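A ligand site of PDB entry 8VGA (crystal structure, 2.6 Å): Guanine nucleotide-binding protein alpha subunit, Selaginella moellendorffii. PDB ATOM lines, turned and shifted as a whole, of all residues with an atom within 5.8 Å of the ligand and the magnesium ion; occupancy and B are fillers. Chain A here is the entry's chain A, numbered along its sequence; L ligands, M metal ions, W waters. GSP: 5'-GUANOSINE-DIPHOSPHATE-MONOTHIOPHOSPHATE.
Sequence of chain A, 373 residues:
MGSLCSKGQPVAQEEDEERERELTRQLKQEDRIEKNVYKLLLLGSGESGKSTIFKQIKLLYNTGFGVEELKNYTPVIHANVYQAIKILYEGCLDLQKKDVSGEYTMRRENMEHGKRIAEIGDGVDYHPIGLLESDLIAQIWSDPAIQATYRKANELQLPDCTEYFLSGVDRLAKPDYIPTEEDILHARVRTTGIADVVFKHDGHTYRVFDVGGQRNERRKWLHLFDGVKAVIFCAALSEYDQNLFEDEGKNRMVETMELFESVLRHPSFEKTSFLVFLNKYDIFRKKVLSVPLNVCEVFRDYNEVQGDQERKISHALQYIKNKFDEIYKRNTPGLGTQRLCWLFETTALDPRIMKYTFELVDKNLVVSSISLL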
ATOM      1  N   GLY A  44     -19.658  -3.026 -14.476  1.00  0.00           N
ATOM      2  CA  GLY A  44     -20.417  -3.560 -15.592  1.00  0.00           C
ATOM      3  C   GLY A  44     -20.611  -2.462 -16.606  1.00  0.00           C
ATOM      4  O   GLY A  44     -20.306  -1.304 -16.356  1.00  0.00           O
ATOM      5  N   SER A  45     -21.100  -2.850 -17.785  1.00  0.00           N
ATOM      6  CA  SER A  45     -21.272  -1.878 -18.857  1.00  0.00           C
ATOM      7  C   SER A  45     -22.474  -0.980 -18.568  1.00  0.00           C
ATOM      8  O   SER A  45     -23.176  -1.125 -17.564  1.00  0.00           O
ATOM      9  CB  SER A  45     -21.424  -2.591 -20.198  1.00  0.00           C
ATOM     10  OG  SER A  45     -22.665  -3.252 -20.250  1.00  0.00           O
ATOM     11  N   GLY A  46     -22.702  -0.019 -19.450  1.00  0.00           N
ATOM     12  CA  GLY A  46     -23.693   0.996 -19.156  1.00  0.00           C
ATOM     13  C   GLY A  46     -25.092   0.430 -19.195  1.00  0.00           C
ATOM     14  O   GLY A  46     -25.434  -0.375 -20.065  1.00  0.00           O
ATOM     15  N   GLU A  47     -25.915   0.869 -18.239  1.00  0.00           N
ATOM     16  CA  GLU A  47     -27.273   0.383 -18.006  1.00  0.00           C
ATOM     17  C   GLU A  47     -27.347  -1.111 -17.690  1.00  0.00           C
ATOM     18  O   GLU A  47     -28.386  -1.734 -17.931  1.00  0.00           O
ATOM     19  CB  GLU A  47     -28.199   0.714 -19.183  1.00  0.00           C
ATOM     20  CG  GLU A  47     -28.183   2.163 -19.543  1.00  0.00           C
ATOM     21  CD  GLU A  47     -28.833   2.445 -20.871  1.00  0.00           C
ATOM     22  OE1 GLU A  47     -28.133   2.464 -21.889  1.00  0.00           O
ATOM     23  OE2 GLU A  47     -30.032   2.729 -20.894  1.00  0.00           O
ATOM     24  N   SER A  48     -26.278  -1.722 -17.150  1.00  0.00           N
ATOM     25  CA  SER A  48     -26.375  -3.098 -16.685  1.00  0.00           C
ATOM     26  C   SER A  48     -27.182  -3.196 -15.394  1.00  0.00           C
ATOM     27  O   SER A  48     -27.738  -4.265 -15.111  1.00  0.00           O
ATOM     28  CB  SER A  48     -24.978  -3.706 -16.490  1.00  0.00           C
ATOM     29  OG  SER A  48     -24.153  -2.889 -15.668  1.00  0.00           O
ATOM     30  N   GLY A  49     -27.257  -2.109 -14.619  1.00  0.00           N
ATOM     31  CA  GLY A  49     -28.052  -2.053 -13.402  1.00  0.00           C
ATOM     32  C   GLY A  49     -27.298  -1.630 -12.141  1.00  0.00           C
ATOM     33  O   GLY A  49     -27.883  -1.654 -11.045  1.00  0.00           O
ATOM     34  N   LYS A  50     -26.029  -1.236 -12.260  1.00  0.00           N
ATOM     35  CA  LYS A  50     -25.200  -0.971 -11.072  1.00  0.00           C
ATOM     36  C   LYS A  50     -25.824   0.061 -10.136  1.00  0.00           C
ATOM     37  O   LYS A  50     -25.846  -0.134  -8.914  1.00  0.00           O
ATOM     38  CB  LYS A  50     -23.804  -0.521 -11.480  1.00  0.00           C
ATOM     39  CG  LYS A  50     -23.100  -1.436 -12.464  1.00  0.00           C
ATOM     40  CD  LYS A  50     -21.794  -0.825 -12.999  1.00  0.00           C
ATOM     41  CE  LYS A  50     -22.052   0.475 -13.783  1.00  0.00           C
ATOM     42  NZ  LYS A  50     -22.626   0.179 -15.114  1.00  0.00           N
ATOM     43  N   SER A  51     -26.333   1.171 -10.678  1.00  0.00           N
ATOM     44  CA  SER A  51     -26.924   2.171  -9.811  1.00  0.00           C
ATOM     45  C   SER A  51     -28.238   1.688  -9.192  1.00  0.00           C
ATOM     46  O   SER A  51     -28.532   2.043  -8.040  1.00  0.00           O
ATOM     47  CB  SER A  51     -27.140   3.476 -10.577  1.00  0.00           C
ATOM     48  OG  SER A  51     -25.898   4.139 -10.757  1.00  0.00           O
ATOM     49  N   THR A  52     -29.041   0.913  -9.926  1.00  0.00           N
ATOM     50  CA  THR A  52     -30.254   0.357  -9.334  1.00  0.00           C
ATOM     51  C   THR A  52     -29.927  -0.574  -8.170  1.00  0.00           C
ATOM     52  O   THR A  52     -30.605  -0.545  -7.130  1.00  0.00           O
ATOM     53  CB  THR A  52     -31.051  -0.391 -10.402  1.00  0.00           C
ATOM     54  OG1 THR A  52     -31.150   0.405 -11.585  1.00  0.00           O
ATOM     55  CG2 THR A  52     -32.448  -0.746  -9.887  1.00  0.00           C
ATOM     56  N   ILE A  53     -28.877  -1.394  -8.312  1.00  0.00           N
ATOM     57  CA  ILE A  53     -28.437  -2.222  -7.204  1.00  0.00           C
ATOM     58  C   ILE A  53     -27.955  -1.351  -6.054  1.00  0.00           C
ATOM     59  O   ILE A  53     -28.242  -1.618  -4.880  1.00  0.00           O
ATOM     60  CB  ILE A  53     -27.350  -3.215  -7.662  1.00  0.00           C
ATOM     61  CG1 ILE A  53     -28.021  -4.435  -8.293  1.00  0.00           C
ATOM     62  CG2 ILE A  53     -26.548  -3.712  -6.488  1.00  0.00           C
ATOM     63  CD1 ILE A  53     -27.265  -4.980  -9.449  1.00  0.00           C
ATOM     64  N   ASP A 160     -35.169   2.078 -20.156  1.00  0.00           N
ATOM     65  CA  ASP A 160     -35.946   0.894 -19.784  1.00  0.00           C
ATOM     66  C   ASP A 160     -37.238   1.255 -19.049  1.00  0.00           C
ATOM     67  O   ASP A 160     -38.235   0.542 -19.172  1.00  0.00           O
ATOM     68  CB  ASP A 160     -35.099  -0.048 -18.926  1.00  0.00           C
ATOM     69  CG  ASP A 160     -33.995  -0.711 -19.709  1.00  0.00           C
ATOM     70  OD1 ASP A 160     -32.810  -0.318 -19.529  1.00  0.00           O
ATOM     71  OD2 ASP A 160     -34.327  -1.615 -20.524  1.00  0.00           O
ATOM     72  N   CYS A 161     -37.241   2.350 -18.312  1.00  0.00           N
ATOM     73  CA  CYS A 161     -38.406   2.805 -17.551  1.00  0.00           C
ATOM     74  C   CYS A 161     -39.519   3.406 -18.436  1.00  0.00           C
ATOM     75  O   CYS A 161     -40.496   3.956 -17.879  1.00  0.00           O
ATOM     76  CB  CYS A 161     -37.949   3.843 -16.530  1.00  0.00           C
ATOM     77  SG  CYS A 161     -37.156   5.292 -17.305  1.00  0.00           S
ATOM     78  N   LEU A 185     -36.229   3.609  -8.147  1.00  0.00           N
ATOM     79  CA  LEU A 185     -35.487   2.499  -8.725  1.00  0.00           C
ATOM     80  C   LEU A 185     -35.614   2.476 -10.249  1.00  0.00           C
ATOM     81  O   LEU A 185     -34.657   2.101 -10.938  1.00  0.00           O
ATOM     82  CB  LEU A 185     -35.959   1.187  -8.117  1.00  0.00           C
ATOM     83  CG  LEU A 185     -35.639   1.096  -6.620  1.00  0.00           C
ATOM     84  CD1 LEU A 185     -36.665   0.213  -5.905  1.00  0.00           C
ATOM     85  CD2 LEU A 185     -34.214   0.596  -6.381  1.00  0.00           C
ATOM     86  N   HIS A 186     -36.768   2.884 -10.783  1.00  0.00           N
ATOM     87  CA  HIS A 186     -36.954   2.957 -12.226  1.00  0.00           C
ATOM     88  C   HIS A 186     -36.234   4.146 -12.857  1.00  0.00           C
ATOM     89  O   HIS A 186     -35.858   4.083 -14.026  1.00  0.00           O
ATOM     90  CB  HIS A 186     -38.440   3.076 -12.568  1.00  0.00           C
ATOM     91  CG  HIS A 186     -39.132   1.764 -12.751  1.00  0.00           C
ATOM     92  ND1 HIS A 186     -39.796   1.126 -11.717  1.00  0.00           N
ATOM     93  CD2 HIS A 186     -39.286   0.970 -13.831  1.00  0.00           C
ATOM     94  CE1 HIS A 186     -40.317   0.000 -12.158  1.00  0.00           C
ATOM     95  NE2 HIS A 186     -40.022  -0.125 -13.437  1.00  0.00           N
ATOM     96  N   ALA A 187     -36.077   5.242 -12.098  1.00  0.00           N
ATOM     97  CA  ALA A 187     -35.526   6.473 -12.648  1.00  0.00           C
ATOM     98  C   ALA A 187     -34.106   6.229 -13.152  1.00  0.00           C
ATOM     99  O   ALA A 187     -33.327   5.468 -12.563  1.00  0.00           O
ATOM    100  CB  ALA A 187     -35.534   7.570 -11.596  1.00  0.00           C
ATOM    101  N   ARG A 188     -33.777   6.872 -14.262  1.00  0.00           N
ATOM    102  CA  ARG A 188     -32.599   6.588 -15.061  1.00  0.00           C
ATOM    103  C   ARG A 188     -31.699   7.833 -15.056  1.00  0.00           C
ATOM    104  O   ARG A 188     -32.069   8.867 -15.627  1.00  0.00           O
ATOM    105  CB  ARG A 188     -33.001   6.214 -16.486  1.00  0.00           C
ATOM    106  CG  ARG A 188     -31.869   6.314 -17.489  1.00  0.00           C
ATOM    107  CD  ARG A 188     -30.825   5.298 -17.209  1.00  0.00           C
ATOM    108  NE  ARG A 188     -29.682   5.532 -18.091  1.00  0.00           N
ATOM    109  CZ  ARG A 188     -28.456   5.063 -17.866  1.00  0.00           C
ATOM    110  NH1 ARG A 188     -28.207   4.297 -16.804  1.00  0.00           N
ATOM    111  NH2 ARG A 188     -27.485   5.357 -18.715  1.00  0.00           N
ATOM    112  N   VAL A 189     -30.549   7.722 -14.415  1.00  0.00           N
ATOM    113  CA  VAL A 189     -29.514   8.740 -14.401  1.00  0.00           C
ATOM    114  C   VAL A 189     -28.228   8.101 -14.904  1.00  0.00           C
ATOM    115  O   VAL A 189     -27.744   7.127 -14.311  1.00  0.00           O
ATOM    116  CB  VAL A 189     -29.276   9.315 -12.998  1.00  0.00           C
ATOM    117  CG1 VAL A 189     -28.101  10.282 -13.017  1.00  0.00           C
ATOM    118  CG2 VAL A 189     -30.519   9.984 -12.457  1.00  0.00           C
ATOM    119  N   ARG A 190     -27.672   8.655 -15.967  1.00  0.00           N
ATOM    120  CA  ARG A 190     -26.434   8.117 -16.523  1.00  0.00           C
ATOM    121  C   ARG A 190     -25.283   8.531 -15.608  1.00  0.00           C
ATOM    122  O   ARG A 190     -24.946   9.705 -15.520  1.00  0.00           O
ATOM    123  CB  ARG A 190     -26.258   8.612 -17.959  1.00  0.00           C
ATOM    124  CG  ARG A 190     -24.907   8.399 -18.608  1.00  0.00           C
ATOM    125  CD  ARG A 190     -24.872   9.082 -19.981  1.00  0.00           C
ATOM    126  NE  ARG A 190     -23.745  10.001 -20.137  1.00  0.00           N
ATOM    127  CZ  ARG A 190     -23.778  11.282 -19.761  1.00  0.00           C
ATOM    128  NH1 ARG A 190     -24.878  11.774 -19.206  1.00  0.00           N
ATOM    129  NH2 ARG A 190     -22.721  12.056 -19.934  1.00  0.00           N
ATOM    130  N   THR A 191     -24.691   7.550 -14.902  1.00  0.00           N
ATOM    131  CA  THR A 191     -23.699   7.860 -13.867  1.00  0.00           C
ATOM    132  C   THR A 191     -22.397   8.411 -14.472  1.00  0.00           C
ATOM    133  O   THR A 191     -21.843   7.827 -15.415  1.00  0.00           O
ATOM    134  CB  THR A 191     -23.409   6.599 -13.041  1.00  0.00           C
ATOM    135  OG1 THR A 191     -24.613   6.188 -12.385  1.00  0.00           O
ATOM    136  CG2 THR A 191     -22.343   6.875 -11.992  1.00  0.00           C
ATOM    137  N   ASP A 210     -20.206   2.899  -6.512  1.00  0.00           N
ATOM    138  CA  ASP A 210     -20.930   2.932  -7.777  1.00  0.00           C
ATOM    139  C   ASP A 210     -20.150   3.810  -8.750  1.00  0.00           C
ATOM    140  O   ASP A 210     -19.699   4.906  -8.390  1.00  0.00           O
ATOM    141  CB  ASP A 210     -22.366   3.437  -7.571  1.00  0.00           C
ATOM    142  CG  ASP A 210     -23.191   3.444  -8.877  1.00  0.00           C
ATOM    143  OD1 ASP A 210     -22.992   2.559  -9.735  1.00  0.00           O
ATOM    144  OD2 ASP A 210     -24.066   4.338  -9.051  1.00  0.00           O
ATOM    145  N   VAL A 211     -19.997   3.335  -9.974  1.00  0.00           N
ATOM    146  CA  VAL A 211     -19.295   4.078 -11.009  1.00  0.00           C
ATOM    147  C   VAL A 211     -20.022   3.836 -12.324  1.00  0.00           C
ATOM    148  O   VAL A 211     -20.737   2.846 -12.483  1.00  0.00           O
ATOM    149  CB  VAL A 211     -17.787   3.669 -11.080  1.00  0.00           C
ATOM    150  CG1 VAL A 211     -17.620   2.205 -11.573  1.00  0.00           C
ATOM    151  CG2 VAL A 211     -16.999   4.638 -11.941  1.00  0.00           C
ATOM    152  N   GLY A 212     -19.875   4.769 -13.252  1.00  0.00           N
ATOM    153  CA  GLY A 212     -20.472   4.610 -14.557  1.00  0.00           C
ATOM    154  C   GLY A 212     -19.790   3.509 -15.361  1.00  0.00           C
ATOM    155  O   GLY A 212     -18.619   3.222 -15.172  1.00  0.00           O
ATOM    156  N   GLY A 213     -20.565   2.897 -16.259  1.00  0.00           N
ATOM    157  CA  GLY A 213     -20.112   1.776 -17.063  1.00  0.00           C
ATOM    158  C   GLY A 213     -20.076   2.037 -18.557  1.00  0.00           C
ATOM    159  O   GLY A 213     -19.657   1.175 -19.346  1.00  0.00           O
ATOM    160  N   GLN A 214     -20.531   3.202 -18.990  1.00  0.00           N
ATOM    161  CA  GLN A 214     -20.327   3.537 -20.387  1.00  0.00           C
ATOM    162  C   GLN A 214     -18.842   3.669 -20.663  1.00  0.00           C
ATOM    163  O   GLN A 214     -18.055   3.966 -19.761  1.00  0.00           O
ATOM    164  CB  GLN A 214     -21.070   4.810 -20.759  1.00  0.00           C
ATOM    165  CG  GLN A 214     -22.557   4.644 -20.766  1.00  0.00           C
ATOM    166  CD  GLN A 214     -23.276   5.912 -21.165  1.00  0.00           C
ATOM    167  OE1 GLN A 214     -22.702   7.007 -21.156  1.00  0.00           O
ATOM    168  NE2 GLN A 214     -24.543   5.766 -21.503  1.00  0.00           N
ATOM    169  N   CYS A 234     -22.253  -6.481 -12.727  1.00  0.00           N
ATOM    170  CA  CYS A 234     -23.614  -6.500 -13.243  1.00  0.00           C
ATOM    171  C   CYS A 234     -23.593  -6.747 -14.733  1.00  0.00           C
ATOM    172  O   CYS A 234     -22.843  -6.088 -15.469  1.00  0.00           O
ATOM    173  CB  CYS A 234     -24.325  -5.194 -12.946  1.00  0.00           C
ATOM    174  SG  CYS A 234     -24.338  -4.900 -11.218  1.00  0.00           S
ATOM    175  N   ASN A 279     -28.517  -9.546 -14.293  1.00  0.00           N
ATOM    176  CA  ASN A 279     -29.597  -8.646 -13.930  1.00  0.00           C
ATOM    177  C   ASN A 279     -30.624  -8.570 -15.045  1.00  0.00           C
ATOM    178  O   ASN A 279     -30.440  -9.122 -16.139  1.00  0.00           O
ATOM    179  CB  ASN A 279     -29.005  -7.248 -13.642  1.00  0.00           C
ATOM    180  CG  ASN A 279     -29.995  -6.343 -12.982  1.00  0.00           C
ATOM    181  OD1 ASN A 279     -30.765  -6.781 -12.153  1.00  0.00           O
ATOM    182  ND2 ASN A 279     -29.992  -5.059 -13.369  1.00  0.00           N
ATOM    183  N   LYS A 280     -31.722  -7.860 -14.768  1.00  0.00           N
ATOM    184  CA  LYS A 280     -32.842  -7.709 -15.709  1.00  0.00           C
ATOM    185  C   LYS A 280     -33.435  -9.065 -16.074  1.00  0.00           C
ATOM    186  O   LYS A 280     -33.896  -9.290 -17.208  1.00  0.00           O
ATOM    187  CB  LYS A 280     -32.425  -6.916 -16.949  1.00  0.00           C
ATOM    188  CG  LYS A 280     -32.128  -5.467 -16.613  1.00  0.00           C
ATOM    189  CD  LYS A 280     -31.717  -4.629 -17.799  1.00  0.00           C
ATOM    190  CE  LYS A 280     -31.679  -3.155 -17.389  1.00  0.00           C
ATOM    191  NZ  LYS A 280     -31.113  -2.263 -18.430  1.00  0.00           N
ATOM    192  N   TYR A 281     -33.432  -9.993 -15.105  1.00  0.00           N
ATOM    193  CA  TYR A 281     -34.044 -11.301 -15.298  1.00  0.00           C
ATOM    194  C   TYR A 281     -35.516 -11.172 -15.679  1.00  0.00           C
ATOM    195  O   TYR A 281     -36.015 -11.948 -16.505  1.00  0.00           O
ATOM    196  CB  TYR A 281     -33.865 -12.135 -14.023  1.00  0.00           C
ATOM    197  CG  TYR A 281     -34.552 -13.459 -14.063  1.00  0.00           C
ATOM    198  CD1 TYR A 281     -34.164 -14.436 -14.965  1.00  0.00           C
ATOM    199  CD2 TYR A 281     -35.611 -13.730 -13.187  1.00  0.00           C
ATOM    200  CE1 TYR A 281     -34.814 -15.678 -15.003  1.00  0.00           C
ATOM    201  CE2 TYR A 281     -36.263 -14.967 -13.217  1.00  0.00           C
ATOM    202  CZ  TYR A 281     -35.870 -15.936 -14.123  1.00  0.00           C
ATOM    203  OH  TYR A 281     -36.510 -17.163 -14.168  1.00  0.00           O
ATOM    204  N   ASP A 282     -36.235 -10.200 -15.103  1.00  0.00           N
ATOM    205  CA  ASP A 282     -37.660  -9.981 -15.449  1.00  0.00           C
ATOM    206  C   ASP A 282     -37.845  -9.691 -16.937  1.00  0.00           C
ATOM    207  O   ASP A 282     -38.751 -10.262 -17.573  1.00  0.00           O
ATOM    208  CB  ASP A 282     -38.246  -8.836 -14.604  1.00  0.00           C
ATOM    209  CG  ASP A 282     -37.654  -7.458 -14.962  1.00  0.00           C
ATOM    210  OD1 ASP A 282     -36.433  -7.374 -15.263  1.00  0.00           O
ATOM    211  OD2 ASP A 282     -38.382  -6.436 -14.883  1.00  0.00           O
ATOM    212  N   ILE A 283     -37.003  -8.823 -17.524  1.00  0.00           N
ATOM    213  CA  ILE A 283     -37.104  -8.523 -18.952  1.00  0.00           C
ATOM    214  C   ILE A 283     -36.711  -9.744 -19.777  1.00  0.00           C
ATOM    215  O   ILE A 283     -37.386 -10.094 -20.752  1.00  0.00           O
ATOM    216  CB  ILE A 283     -36.241  -7.304 -19.316  1.00  0.00           C
ATOM    217  CG1 ILE A 283     -36.653  -6.064 -18.509  1.00  0.00           C
ATOM    218  CG2 ILE A 283     -36.342  -6.997 -20.810  1.00  0.00           C
ATOM    219  CD1 ILE A 283     -35.722  -4.875 -18.728  1.00  0.00           C
ATOM    220  N   THR A 346     -31.018 -11.954 -11.290  1.00  0.00           N
ATOM    221  CA  THR A 346     -31.523 -10.920 -10.416  1.00  0.00           C
ATOM    222  C   THR A 346     -32.455 -10.001 -11.179  1.00  0.00           C
ATOM    223  O   THR A 346     -32.421  -9.929 -12.415  1.00  0.00           O
ATOM    224  CB  THR A 346     -30.394 -10.054  -9.829  1.00  0.00           C
ATOM    225  OG1 THR A 346     -29.742  -9.288 -10.865  1.00  0.00           O
ATOM    226  CG2 THR A 346     -29.387 -10.899  -9.049  1.00  0.00           C
ATOM    227  N   THR A 347     -33.273  -9.284 -10.430  1.00  0.00           N
ATOM    228  CA  THR A 347     -34.008  -8.128 -10.942  1.00  0.00           C
ATOM    229  C   THR A 347     -33.767  -6.992  -9.960  1.00  0.00           C
ATOM    230  O   THR A 347     -34.288  -7.011  -8.842  1.00  0.00           O
ATOM    231  CB  THR A 347     -35.493  -8.465 -11.128  1.00  0.00           C
ATOM    232  OG1 THR A 347     -35.604  -9.481 -12.137  1.00  0.00           O
ATOM    233  CG2 THR A 347     -36.321  -7.252 -11.528  1.00  0.00           C
ATOM    234  N   ALA A 348     -32.939  -6.016 -10.378  1.00  0.00           N
ATOM    235  CA  ALA A 348     -32.453  -4.993  -9.450  1.00  0.00           C
ATOM    236  C   ALA A 348     -33.599  -4.148  -8.894  1.00  0.00           C
ATOM    237  O   ALA A 348     -33.503  -3.658  -7.759  1.00  0.00           O
ATOM    238  CB  ALA A 348     -31.412  -4.118 -10.132  1.00  0.00           C
ATOM    239  N   LEU A 349     -34.691  -3.991  -9.651  1.00  0.00           N
ATOM    240  CA  LEU A 349     -35.843  -3.219  -9.170  1.00  0.00           C
ATOM    241  C   LEU A 349     -36.563  -3.885  -8.008  1.00  0.00           C
ATOM    242  O   LEU A 349     -37.240  -3.202  -7.230  1.00  0.00           O
ATOM    243  CB  LEU A 349     -36.865  -2.975 -10.286  1.00  0.00           C
ATOM    244  CG  LEU A 349     -36.436  -2.268 -11.576  1.00  0.00           C
ATOM    245  CD1 LEU A 349     -37.486  -2.462 -12.676  1.00  0.00           C
ATOM    246  CD2 LEU A 349     -36.209  -0.826 -11.275  1.00  0.00           C
HETATM  247  PG  GSP L   1     -24.504   3.462 -16.017  1.00  0.00           P
HETATM  248  O3B GSP L   1     -25.758   2.456 -15.952  1.00  0.00           O
HETATM  249  S1G GSP L   1     -24.716   4.415 -17.475  1.00  0.00           S
HETATM  250  O2G GSP L   1     -23.179   2.663 -16.039  1.00  0.00           O
HETATM  251  O3G GSP L   1     -24.489   4.277 -14.724  1.00  0.00           O
HETATM  252  PB  GSP L   1     -26.086   1.520 -14.684  1.00  0.00           P
HETATM  253  O1B GSP L   1     -25.387   0.196 -14.739  1.00  0.00           O
HETATM  254  O2B GSP L   1     -25.870   2.245 -13.410  1.00  0.00           O
HETATM  255  PA  GSP L   1     -28.871   1.732 -14.139  1.00  0.00           P
HETATM  256  O1A GSP L   1     -28.752   1.317 -12.729  1.00  0.00           O
HETATM  257  O2A GSP L   1     -29.007   3.216 -14.226  1.00  0.00           O
HETATM  258  O3A GSP L   1     -27.638   1.147 -14.982  1.00  0.00           O
HETATM  259  O5' GSP L   1     -30.066   1.006 -14.918  1.00  0.00           O
HETATM  260  C5' GSP L   1     -30.563   1.567 -16.106  1.00  0.00           C
HETATM  261  C4' GSP L   1     -32.078   1.525 -16.067  1.00  0.00           C
HETATM  262  O4' GSP L   1     -32.533   0.187 -16.145  1.00  0.00           O
HETATM  263  C3' GSP L   1     -32.660   2.142 -14.810  1.00  0.00           C
HETATM  264  O3' GSP L   1     -33.724   2.956 -15.228  1.00  0.00           O
HETATM  265  C2' GSP L   1     -33.267   0.983 -14.065  1.00  0.00           C
HETATM  266  O2' GSP L   1     -34.527   1.337 -13.561  1.00  0.00           O
HETATM  267  C1' GSP L   1     -33.473  -0.082 -15.123  1.00  0.00           C
HETATM  268  N9  GSP L   1     -33.214  -1.410 -14.552  1.00  0.00           N
HETATM  269  C8  GSP L   1     -32.121  -1.758 -13.802  1.00  0.00           C
HETATM  270  N7  GSP L   1     -32.246  -3.070 -13.460  1.00  0.00           N
HETATM  271  C5  GSP L   1     -33.391  -3.563 -13.968  1.00  0.00           C
HETATM  272  C6  GSP L   1     -33.983  -4.820 -13.898  1.00  0.00           C
HETATM  273  O6  GSP L   1     -33.453  -5.745 -13.303  1.00  0.00           O
HETATM  274  N1  GSP L   1     -35.181  -5.016 -14.529  1.00  0.00           N
HETATM  275  C2  GSP L   1     -35.790  -3.980 -15.202  1.00  0.00           C
HETATM  276  N2  GSP L   1     -36.960  -4.180 -15.800  1.00  0.00           N
HETATM  277  N3  GSP L   1     -35.193  -2.746 -15.256  1.00  0.00           N
HETATM  278  C4  GSP L   1     -34.014  -2.525 -14.658  1.00  0.00           C
HETATM  279 MG    MG M   1     -25.038   4.113 -12.772  1.00  0.00          MG
HETATM  280  O   HOH W   1     -23.205   3.167 -12.355  1.00  0.00           O
HETATM  281  O   HOH W   2     -21.901   5.803 -17.342  1.00  0.00           O
HETATM  282  O   HOH W   3     -26.763   4.803 -13.435  1.00  0.00           O
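The backbone carbonyl oxygen (O) of His 186 sits close to the side-chain sulfur (SG) of Cys 161 (3.7 Å).
The backbone carbonyl oxygen (O) of Ser 45 lies within hydrogen-bond range of the side-chain amino group (NZ) of Lys 50, 2.8 Å away.
The side-chain carboxylate (OE2) of Glu 47 is in salt-bridge range of the guanidinium group (NE) of Arg 188 (3.98 Å).
The backbone carbonyl oxygen (O) of Glu 47 lies within hydrogen-bond range of the side-chain amino group (NZ) of Lys 280.
The side-chain amide nitrogen of Asn 279 is in hydrogen-bond range of the backbone carbonyl oxygen of Ser 48 (3.0 Å).
OD1 of Asp 160 is in salt-bridge range of NZ of Lys 280.
The backbone carbonyl oxygen (O) of Thr 346 is in hydrogen-bond range of the backbone NH (N) of Lys 280.
The backbone carbonyl oxygen of Ser 45 lies within hydrogen-bond range of the side-chain hydroxyl of Ser 48, at 2.8 Å.
The magnesium ion is bound by water W3 (2.0 Å), O3G of the ligand (2.0 Å), water W1 (2.1 Å), O2B of the ligand (2.1 Å), OG1 of Thr 191 (2.2 Å) and OG of Ser 51 (2.2 Å).
The magnesium ion has six donor atoms within binding distance.
Water W1 lies within hydrogen-bond range of the backbone carbonyl oxygen of Val 211 (2.5 Å) and the side-chain carboxylate of Asp 210 (2.7 Å).
Water W3 bridges O of Val 189 (2.7 Å) and O2A of the ligand (2.9 Å).
Water W2 lies within hydrogen-bond range of O of Thr 191 (2.8 Å), S1G of the ligand (3.1 Å), N of Gln 214 (3.4 Å) and N of Gly 213 (3.4 Å).
Residues that only touch the magnesium ion: Asp 210.
Within 4 Å of the magnesium ion: Ser 51, Thr 191 and Asp 210.
The nearest printed residue that does not touch the magnesium ion is Val 189 (4.3 Å).
The side-chain carboxylate of Asp 160 lies close to an oxygen (O4') of the ligand (3.4 Å).
Ser 45 touches the ligand.
Gly 46 touches the ligand (CA to O2G, 3.6 Å).
Ala 187 touches the ligand.
Gly 212 touches the ligand.
Gln 214 touches the ligand (CG to S1G, 3.9 Å).
Ile 283 touches the ligand.
Thr 347 touches the ligand (CA to O6, 3.4 Å).
Leu 349 touches the ligand.
24 residues have an atom within 4 Å of the ligand: Ser 45, Gly 46, Glu 47, Ser 48, Gly 49, Lys 50, Ser 51, Thr 52, Asp 160, Leu 185, His 186, Ala 187, Arg 188, Thr 191, Gly 212, Gly 213, Gln 214, Asn 279, Lys 280, Asp 282, Ile 283, Thr 347, Ala 348 and Leu 349.
The nearest printed residue that does not touch the ligand is Val 189 (4.1 Å).
O3G of the ligand sits close to N of Thr 191 (3.3 Å).
An oxygen (O1A) of the ligand lies within hydrogen-bond range of the backbone NH (N) of Ser 51, at 3.2 Å.
The backbone NH of Gly 213 sits at hydrogen-bond distance from an oxygen (O2G) of the ligand, 2.6 Å away.
An oxygen (O3') of the ligand is in hydrogen-bond range of the backbone carbonyl oxygen (O) of His 186, 2.7 Å away.
The backbone NH (N) of Lys 50 is in hydrogen-bond range of an oxygen (O1B) of the ligand (2.9 Å).
An oxygen (O1B) of the ligand is in salt-bridge range of the side-chain amino group (NZ) of Lys 50 (2.8 Å).
O of Leu 185 is in hydrogen-bond range of O2' of the ligand (2.7 Å).
The side-chain carboxylate (OD1) of Asp 282 is in hydrogen-bond range of a nitrogen (N1) of the ligand (2.8 Å).
O3B of the ligand lies within hydrogen-bond range of N of Glu 47 (2.8 Å).
An oxygen (O1A) of the ligand sits at hydrogen-bond distance from the backbone NH (N) of Thr 52 (2.8 Å).
The side-chain hydroxyl (OG1) of Thr 52 lies within hydrogen-bond range of an oxygen (O1A) of the ligand (2.8 Å).
O2A of the ligand is in salt-bridge range of NH1 of Arg 188 (2.9 Å).
O1B of the ligand sits at hydrogen-bond distance from N of Gly 49.
N of Ala 348 sits at hydrogen-bond distance from O6 of the ligand.
A nitrogen (N7) of the ligand is in hydrogen-bond range of the side-chain amide nitrogen (ND2) of Asn 279.
The backbone NH (N) of Lys 280 sits at hydrogen-bond distance from an oxygen (O6) of the ligand.
N of Ser 48 is in hydrogen-bond range of O1B of the ligand (3.2 Å).
O1B of the ligand is in hydrogen-bond range of OG of Ser 48, 3.5 Å away.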
